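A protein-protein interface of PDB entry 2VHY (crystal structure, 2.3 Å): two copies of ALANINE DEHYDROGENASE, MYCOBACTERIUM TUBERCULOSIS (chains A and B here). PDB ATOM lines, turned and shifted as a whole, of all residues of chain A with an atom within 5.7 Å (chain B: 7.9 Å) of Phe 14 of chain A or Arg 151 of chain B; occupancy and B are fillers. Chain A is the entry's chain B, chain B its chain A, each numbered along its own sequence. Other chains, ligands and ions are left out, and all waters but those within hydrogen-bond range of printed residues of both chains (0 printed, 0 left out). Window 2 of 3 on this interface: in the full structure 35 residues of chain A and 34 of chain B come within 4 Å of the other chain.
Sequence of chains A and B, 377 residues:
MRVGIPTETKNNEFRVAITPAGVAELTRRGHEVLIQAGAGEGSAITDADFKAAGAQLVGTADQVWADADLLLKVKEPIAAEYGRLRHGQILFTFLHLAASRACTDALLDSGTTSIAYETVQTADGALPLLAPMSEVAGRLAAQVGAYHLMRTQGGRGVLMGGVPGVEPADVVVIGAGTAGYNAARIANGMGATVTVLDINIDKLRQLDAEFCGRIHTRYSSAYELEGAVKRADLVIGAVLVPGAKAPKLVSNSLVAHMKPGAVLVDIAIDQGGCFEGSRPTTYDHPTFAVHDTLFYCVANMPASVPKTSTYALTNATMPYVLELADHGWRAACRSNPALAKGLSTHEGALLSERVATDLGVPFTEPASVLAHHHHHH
No position is printed for both chains.
O of Leu 149 of chain B is in hydrogen-bond range of N of Gly 157 of chain B (2.8 Å).
The backbone carbonyl oxygen (O) of Met 150 of chain B sits at hydrogen-bond distance from the backbone NH (N) of Gly 155 of chain B, 3.2 Å away.
The backbone carbonyl oxygen of Phe 14 of chain A lies close to the backbone NH of Ser 43 of chain A, at 3.4 Å.
O of Pro 306 of chain A sits at hydrogen-bond distance from OG1 of Thr 310 of chain A (3.0 Å).
Among the printed residues, no Asp or Glu carboxylate lies within 4 Å of a Lys or Arg side-chain nitrogen of the other chain.
O of Ser 304 of chain A is in hydrogen-bond range of N of Arg 151 of chain B (2.9 Å).
Phe 14 of chain A touches Arg 151 of chain B.
Ser 304 of chain A touches Met 150 of chain B.
C of Val 305 of chain A touches O of Gly 157 of chain B, at 3.4 Å.
Val 158 of chain B touches Val 305 of chain A.
CB of Arg 151 of chain B touches CD of Pro 306 of chain A, at 3.6 Å.
Pro 306 of chain A touches Gly 157 of chain B.
Of chain B, only Arg 151 (3.2 Å) comes within 4 Å of Phe 14 of chain A.
Of the printed residues of chain B, Val 305 of chain A touches Gly 157 (3.4 Å) and Val 158 (3.9 Å).
Printed residues of chain A within 4 Å of Met 150 of chain B: Ser 304.
Of the printed residues of chain B, Ser 304 of chain A touches Met 150 and Arg 151.
The nearest residue of chain B that does not touch Phe 14 of chain A is Thr 152 of chain B (4.6 Å).
The nearest residue of chain A that does not touch Arg 151 of chain B is Gly 42 of chain A (4.2 Å).
The nearest printed residue of chain A that does not touch Met 150 of chain B is Val 305 of chain A (4.2 Å).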
ATOM      1  N   GLU A   8      15.670  13.329  -0.320  1.00  0.00           N
ATOM      2  CA  GLU A   8      14.389  13.927   0.023  1.00  0.00           C
ATOM      3  C   GLU A   8      14.680  15.240   0.698  1.00  0.00           C
ATOM      4  O   GLU A   8      15.398  15.290   1.696  1.00  0.00           O
ATOM      5  CB  GLU A   8      13.599  13.010   0.956  1.00  0.00           C
ATOM      6  CG  GLU A   8      13.285  11.645   0.328  1.00  0.00           C
ATOM      7  CD  GLU A   8      12.436  11.746  -0.932  1.00  0.00           C
ATOM      8  OE1 GLU A   8      12.625  10.903  -1.843  1.00  0.00           O
ATOM      9  OE2 GLU A   8      11.581  12.663  -0.993  1.00  0.00           O
ATOM     10  N   ASN A  12      11.504  17.182   7.788  1.00  0.00           N
ATOM     11  CA  ASN A  12      11.428  16.023   8.658  1.00  0.00           C
ATOM     12  C   ASN A  12      11.348  14.708   7.884  1.00  0.00           C
ATOM     13  O   ASN A  12      10.864  13.702   8.414  1.00  0.00           O
ATOM     14  CB  ASN A  12      10.211  16.170   9.585  1.00  0.00           C
ATOM     15  CG  ASN A  12       9.643  17.604   9.605  1.00  0.00           C
ATOM     16  OD1 ASN A  12      10.328  18.560   9.983  1.00  0.00           O
ATOM     17  ND2 ASN A  12       8.386  17.747   9.187  1.00  0.00           N
ATOM     18  N   GLU A  13      11.830  14.723   6.640  1.00  0.00           N
ATOM     19  CA  GLU A  13      11.831  13.537   5.777  1.00  0.00           C
ATOM     20  C   GLU A  13      13.230  12.936   5.659  1.00  0.00           C
ATOM     21  O   GLU A  13      14.098  13.495   4.996  1.00  0.00           O
ATOM     22  CB  GLU A  13      11.314  13.898   4.382  1.00  0.00           C
ATOM     23  CG  GLU A  13      11.149  12.711   3.451  1.00  0.00           C
ATOM     24  CD  GLU A  13      10.345  11.569   4.075  1.00  0.00           C
ATOM     25  OE1 GLU A  13       9.205  11.799   4.536  1.00  0.00           O
ATOM     26  OE2 GLU A  13      10.861  10.432   4.099  1.00  0.00           O
ATOM     27  N   PHE A  14      13.438  11.788   6.298  1.00  0.00           N
ATOM     28  CA  PHE A  14      14.738  11.118   6.287  1.00  0.00           C
ATOM     29  C   PHE A  14      14.738   9.795   5.515  1.00  0.00           C
ATOM     30  O   PHE A  14      15.596   8.947   5.742  1.00  0.00           O
ATOM     31  CB  PHE A  14      15.189  10.824   7.720  1.00  0.00           C
ATOM     32  CG  PHE A  14      14.937  11.941   8.686  1.00  0.00           C
ATOM     33  CD1 PHE A  14      15.726  13.088   8.670  1.00  0.00           C
ATOM     34  CD2 PHE A  14      13.911  11.842   9.621  1.00  0.00           C
ATOM     35  CE1 PHE A  14      15.501  14.124   9.579  1.00  0.00           C
ATOM     36  CE2 PHE A  14      13.677  12.866  10.530  1.00  0.00           C
ATOM     37  CZ  PHE A  14      14.476  14.013  10.510  1.00  0.00           C
ATOM     38  N   ARG A  15      13.790   9.608   4.608  1.00  0.00           N
ATOM     39  CA  ARG A  15      13.727   8.360   3.857  1.00  0.00           C
ATOM     40  C   ARG A  15      14.432   8.446   2.497  1.00  0.00           C
ATOM     41  O   ARG A  15      14.857   9.523   2.079  1.00  0.00           O
ATOM     42  CB  ARG A  15      12.256   7.939   3.695  1.00  0.00           C
ATOM     43  CG  ARG A  15      11.533   7.751   5.037  1.00  0.00           C
ATOM     44  CD  ARG A  15      10.066   7.302   4.920  1.00  0.00           C
ATOM     45  NE  ARG A  15       9.171   8.346   4.419  1.00  0.00           N
ATOM     46  CZ  ARG A  15       7.850   8.214   4.295  1.00  0.00           C
ATOM     47  NH1 ARG A  15       7.255   7.084   4.637  1.00  0.00           N
ATOM     48  NH2 ARG A  15       7.122   9.213   3.811  1.00  0.00           N
ATOM     49  N   VAL A  16      14.580   7.299   1.835  1.00  0.00           N
ATOM     50  CA  VAL A  16      15.212   7.221   0.520  1.00  0.00           C
ATOM     51  C   VAL A  16      14.464   6.219  -0.371  1.00  0.00           C
ATOM     52  O   VAL A  16      14.087   5.128   0.070  1.00  0.00           O
ATOM     53  CB  VAL A  16      16.728   6.836   0.608  1.00  0.00           C
ATOM     54  CG1 VAL A  16      16.919   5.549   1.380  1.00  0.00           C
ATOM     55  CG2 VAL A  16      17.301   6.683  -0.789  1.00  0.00           C
ATOM     56  N   ALA A  39      21.827  10.841   0.272  1.00  0.00           N
ATOM     57  CA  ALA A  39      20.414  10.558   0.031  1.00  0.00           C
ATOM     58  C   ALA A  39      19.901   9.525   1.034  1.00  0.00           C
ATOM     59  O   ALA A  39      18.842   9.714   1.652  1.00  0.00           O
ATOM     60  CB  ALA A  39      20.224  10.048  -1.395  1.00  0.00           C
ATOM     61  N   GLY A  40      20.669   8.439   1.185  1.00  0.00           N
ATOM     62  CA  GLY A  40      20.321   7.371   2.106  1.00  0.00           C
ATOM     63  C   GLY A  40      20.929   7.546   3.489  1.00  0.00           C
ATOM     64  O   GLY A  40      20.520   6.891   4.440  1.00  0.00           O
ATOM     65  N   GLY A  42      20.401   9.578   5.620  1.00  0.00           N
ATOM     66  CA  GLY A  42      19.339   9.889   6.571  1.00  0.00           C
ATOM     67  C   GLY A  42      18.608   8.715   7.202  1.00  0.00           C
ATOM     68  O   GLY A  42      17.996   8.848   8.263  1.00  0.00           O
ATOM     69  N   SER A  43      18.645   7.565   6.543  1.00  0.00           N
ATOM     70  CA  SER A  43      17.994   6.374   7.073  1.00  0.00           C
ATOM     71  C   SER A  43      19.027   5.266   7.285  1.00  0.00           C
ATOM     72  O   SER A  43      18.790   4.100   6.964  1.00  0.00           O
ATOM     73  CB  SER A  43      16.882   5.907   6.125  1.00  0.00           C
ATOM     74  OG  SER A  43      17.350   5.760   4.801  1.00  0.00           O
ATOM     75  N   ALA A 303       7.834   8.319   8.720  1.00  0.00           N
ATOM     76  CA  ALA A 303       9.074   9.053   8.602  1.00  0.00           C
ATOM     77  C   ALA A 303       9.773   8.941   9.962  1.00  0.00           C
ATOM     78  O   ALA A 303      10.987   9.140  10.067  1.00  0.00           O
ATOM     79  CB  ALA A 303       8.790  10.509   8.261  1.00  0.00           C
ATOM     80  N   SER A 304       8.997   8.608  10.996  1.00  0.00           N
ATOM     81  CA  SER A 304       9.508   8.463  12.362  1.00  0.00           C
ATOM     82  C   SER A 304      10.574   7.370  12.449  1.00  0.00           C
ATOM     83  O   SER A 304      11.502   7.452  13.259  1.00  0.00           O
ATOM     84  CB  SER A 304       8.370   8.103  13.320  1.00  0.00           C
ATOM     85  OG  SER A 304       7.273   8.992  13.219  1.00  0.00           O
ATOM     86  N   VAL A 305      10.424   6.339  11.620  1.00  0.00           N
ATOM     87  CA  VAL A 305      11.358   5.219  11.594  1.00  0.00           C
ATOM     88  C   VAL A 305      11.823   4.926  10.165  1.00  0.00           C
ATOM     89  O   VAL A 305      11.483   3.885   9.598  1.00  0.00           O
ATOM     90  CB  VAL A 305      10.704   3.948  12.219  1.00  0.00           C
ATOM     91  CG1 VAL A 305      10.348   4.218  13.679  1.00  0.00           C
ATOM     92  CG2 VAL A 305       9.450   3.550  11.443  1.00  0.00           C
ATOM     93  N   PRO A 306      12.629   5.843   9.574  1.00  0.00           N
ATOM     94  CA  PRO A 306      13.192   5.774   8.210  1.00  0.00           C
ATOM     95  C   PRO A 306      13.878   4.468   7.807  1.00  0.00           C
ATOM     96  O   PRO A 306      13.562   3.890   6.759  1.00  0.00           O
ATOM     97  CB  PRO A 306      14.147   6.971   8.165  1.00  0.00           C
ATOM     98  CG  PRO A 306      14.492   7.201   9.593  1.00  0.00           C
ATOM     99  CD  PRO A 306      13.173   7.018  10.281  1.00  0.00           C
ATOM    100  N   THR A 310      11.900   2.986   4.950  1.00  0.00           N
ATOM    101  CA  THR A 310      12.557   3.034   3.637  1.00  0.00           C
ATOM    102  C   THR A 310      12.529   1.641   3.035  1.00  0.00           C
ATOM    103  O   THR A 310      12.071   1.453   1.919  1.00  0.00           O
ATOM    104  CB  THR A 310      14.034   3.474   3.727  1.00  0.00           C
ATOM    105  OG1 THR A 310      14.092   4.871   4.007  1.00  0.00           O
ATOM    106  CG2 THR A 310      14.768   3.201   2.415  1.00  0.00           C
ATOM    107  N   ALA B 146      11.842   2.012  23.125  1.00  0.00           N
ATOM    108  CA  ALA B 146      11.232   1.835  21.813  1.00  0.00           C
ATOM    109  C   ALA B 146      10.803   3.195  21.265  1.00  0.00           C
ATOM    110  O   ALA B 146      10.731   3.408  20.050  1.00  0.00           O
ATOM    111  CB  ALA B 146      10.022   0.922  21.922  1.00  0.00           C
ATOM    112  N   TYR B 147      10.523   4.114  22.182  1.00  0.00           N
ATOM    113  CA  TYR B 147      10.082   5.441  21.821  1.00  0.00           C
ATOM    114  C   TYR B 147      11.216   6.362  21.424  1.00  0.00           C
ATOM    115  O   TYR B 147      11.135   7.069  20.424  1.00  0.00           O
ATOM    116  CB  TYR B 147       9.314   6.070  22.973  1.00  0.00           C
ATOM    117  CG  TYR B 147       8.575   7.297  22.528  1.00  0.00           C
ATOM    118  CD1 TYR B 147       9.075   8.571  22.776  1.00  0.00           C
ATOM    119  CD2 TYR B 147       7.398   7.179  21.793  1.00  0.00           C
ATOM    120  CE1 TYR B 147       8.418   9.693  22.297  1.00  0.00           C
ATOM    121  CE2 TYR B 147       6.739   8.289  21.313  1.00  0.00           C
ATOM    122  CZ  TYR B 147       7.249   9.539  21.564  1.00  0.00           C
ATOM    123  OH  TYR B 147       6.582  10.629  21.065  1.00  0.00           O
ATOM    124  N   HIS B 148      12.278   6.373  22.213  1.00  0.00           N
ATOM    125  CA  HIS B 148      13.397   7.227  21.882  1.00  0.00           C
ATOM    126  C   HIS B 148      14.244   6.692  20.731  1.00  0.00           C
ATOM    127  O   HIS B 148      15.198   7.344  20.306  1.00  0.00           O
ATOM    128  CB  HIS B 148      14.222   7.481  23.134  1.00  0.00           C
ATOM    129  CG  HIS B 148      13.494   8.305  24.147  1.00  0.00           C
ATOM    130  ND1 HIS B 148      14.136   9.106  25.063  1.00  0.00           N
ATOM    131  CD2 HIS B 148      12.169   8.495  24.344  1.00  0.00           C
ATOM    132  CE1 HIS B 148      13.237   9.760  25.777  1.00  0.00           C
ATOM    133  NE2 HIS B 148      12.036   9.406  25.360  1.00  0.00           N
ATOM    134  N   LEU B 149      13.872   5.520  20.213  1.00  0.00           N
ATOM    135  CA  LEU B 149      14.568   4.891  19.088  1.00  0.00           C
ATOM    136  C   LEU B 149      14.147   5.572  17.788  1.00  0.00           C
ATOM    137  O   LEU B 149      14.773   5.387  16.745  1.00  0.00           O
ATOM    138  CB  LEU B 149      14.220   3.397  18.998  1.00  0.00           C
ATOM    139  CG  LEU B 149      15.253   2.303  19.300  1.00  0.00           C
ATOM    140  CD1 LEU B 149      14.659   0.931  18.953  1.00  0.00           C
ATOM    141  CD2 LEU B 149      16.514   2.555  18.491  1.00  0.00           C
ATOM    142  N   MET B 150      13.073   6.350  17.853  1.00  0.00           N
ATOM    143  CA  MET B 150      12.570   7.068  16.685  1.00  0.00           C
ATOM    144  C   MET B 150      13.512   8.195  16.267  1.00  0.00           C
ATOM    145  O   MET B 150      13.989   8.974  17.093  1.00  0.00           O
ATOM    146  CB  MET B 150      11.181   7.656  16.967  1.00  0.00           C
ATOM    147  CG  MET B 150      10.058   6.627  17.093  1.00  0.00           C
ATOM    148  SD  MET B 150       8.487   7.369  17.643  1.00  0.00           S
ATOM    149  CE  MET B 150       7.589   7.396  16.149  1.00  0.00           C
ATOM    150  N   ARG B 151      13.764   8.261  14.966  1.00  0.00           N
ATOM    151  CA  ARG B 151      14.632   9.268  14.367  1.00  0.00           C
ATOM    152  C   ARG B 151      14.385  10.663  14.957  1.00  0.00           C
ATOM    153  O   ARG B 151      15.315  11.449  15.176  1.00  0.00           O
ATOM    154  CB  ARG B 151      14.386   9.280  12.856  1.00  0.00           C
ATOM    155  CG  ARG B 151      15.201  10.288  12.116  1.00  0.00           C
ATOM    156  CD  ARG B 151      16.687  10.063  12.325  1.00  0.00           C
ATOM    157  NE  ARG B 151      17.460  11.131  11.703  1.00  0.00           N
ATOM    158  CZ  ARG B 151      17.412  12.403  12.085  1.00  0.00           C
ATOM    159  NH1 ARG B 151      16.630  12.767  13.096  1.00  0.00           N
ATOM    160  NH2 ARG B 151      18.127  13.314  11.440  1.00  0.00           N
ATOM    161  N   THR B 152      13.113  10.944  15.222  1.00  0.00           N
ATOM    162  CA  THR B 152      12.665  12.217  15.776  1.00  0.00           C
ATOM    163  C   THR B 152      12.976  12.412  17.267  1.00  0.00           C
ATOM    164  O   THR B 152      12.742  13.491  17.817  1.00  0.00           O
ATOM    165  CB  THR B 152      11.149  12.380  15.550  1.00  0.00           C
ATOM    166  OG1 THR B 152      10.439  11.368  16.275  1.00  0.00           O
ATOM    167  CG2 THR B 152      10.825  12.228  14.070  1.00  0.00           C
ATOM    168  N   GLN B 153      13.483  11.369  17.920  1.00  0.00           N
ATOM    169  CA  GLN B 153      13.843  11.447  19.335  1.00  0.00           C
ATOM    170  C   GLN B 153      15.354  11.398  19.431  1.00  0.00           C
ATOM    171  O   GLN B 153      15.916  11.245  20.516  1.00  0.00           O
ATOM    172  CB  GLN B 153      13.261  10.265  20.115  1.00  0.00           C
ATOM    173  CG  GLN B 153      11.784  10.373  20.408  1.00  0.00           C
ATOM    174  CD  GLN B 153      11.460  11.585  21.253  1.00  0.00           C
ATOM    175  OE1 GLN B 153      12.047  11.787  22.322  1.00  0.00           O
ATOM    176  NE2 GLN B 153      10.518  12.401  20.784  1.00  0.00           N
ATOM    177  N   GLY B 154      16.004  11.530  18.281  1.00  0.00           N
ATOM    178  CA  GLY B 154      17.450  11.463  18.240  1.00  0.00           C
ATOM    179  C   GLY B 154      17.866  10.045  17.889  1.00  0.00           C
ATOM    180  O   GLY B 154      18.947   9.818  17.341  1.00  0.00           O
ATOM    181  N   GLY B 155      16.986   9.095  18.197  1.00  0.00           N
ATOM    182  CA  GLY B 155      17.248   7.700  17.911  1.00  0.00           C
ATOM    183  C   GLY B 155      17.610   7.431  16.463  1.00  0.00           C
ATOM    184  O   GLY B 155      17.502   8.307  15.601  1.00  0.00           O
ATOM    185  N   ARG B 156      18.028   6.193  16.208  1.00  0.00           N
ATOM    186  CA  ARG B 156      18.446   5.731  14.886  1.00  0.00           C
ATOM    187  C   ARG B 156      17.327   5.734  13.829  1.00  0.00           C
ATOM    188  O   ARG B 156      17.571   6.069  12.667  1.00  0.00           O
ATOM    189  CB  ARG B 156      19.040   4.321  15.030  1.00  0.00           C
ATOM    190  CG  ARG B 156      19.884   3.842  13.851  1.00  0.00           C
ATOM    191  CD  ARG B 156      20.478   2.442  14.107  1.00  0.00           C
ATOM    192  NE  ARG B 156      21.161   1.900  12.928  1.00  0.00           N
ATOM    193  CZ  ARG B 156      22.311   2.362  12.440  1.00  0.00           C
ATOM    194  NH1 ARG B 156      22.927   3.378  13.033  1.00  0.00           N
ATOM    195  NH2 ARG B 156      22.837   1.823  11.347  1.00  0.00           N
ATOM    196  N   GLY B 157      16.109   5.361  14.237  1.00  0.00           N
ATOM    197  CA  GLY B 157      14.968   5.313  13.324  1.00  0.00           C
ATOM    198  C   GLY B 157      14.560   3.883  12.999  1.00  0.00           C
ATOM    199  O   GLY B 157      14.360   3.518  11.841  1.00  0.00           O
ATOM    200  N   VAL B 158      14.426   3.073  14.041  1.00  0.00           N
ATOM    201  CA  VAL B 158      14.080   1.664  13.904  1.00  0.00           C
ATOM    202  C   VAL B 158      12.776   1.308  14.627  1.00  0.00           C
ATOM    203  O   VAL B 158      12.570   1.710  15.782  1.00  0.00           O
ATOM    204  CB  VAL B 158      15.215   0.783  14.507  1.00  0.00           C
ATOM    205  CG1 VAL B 158      15.018  -0.686  14.143  1.00  0.00           C
ATOM    206  CG2 VAL B 158      16.561   1.297  14.050  1.00  0.00           C
ATOM    207  N   GLY B 261      23.293   6.412  16.874  1.00  0.00           N
ATOM    208  CA  GLY B 261      21.846   6.424  17.005  1.00  0.00           C
ATOM    209  C   GLY B 261      21.243   5.403  17.961  1.00  0.00           C
ATOM    210  O   GLY B 261      20.041   5.443  18.247  1.00  0.00           O
ATOM    211  N   LEU B 294      22.098   8.202  22.073  1.00  0.00           N
ATOM    212  CA  LEU B 294      21.000   8.672  22.910  1.00  0.00           C
ATOM    213  C   LEU B 294      21.039   7.925  24.240  1.00  0.00           C
ATOM    214  O   LEU B 294      21.162   6.700  24.280  1.00  0.00           O
ATOM    215  CB  LEU B 294      19.654   8.431  22.202  1.00  0.00           C
ATOM    216  CG  LEU B 294      18.402   9.189  22.675  1.00  0.00           C
ATOM    217  CD1 LEU B 294      17.291   8.979  21.664  1.00  0.00           C
ATOM    218  CD2 LEU B 294      17.966   8.728  24.063  1.00  0.00           C
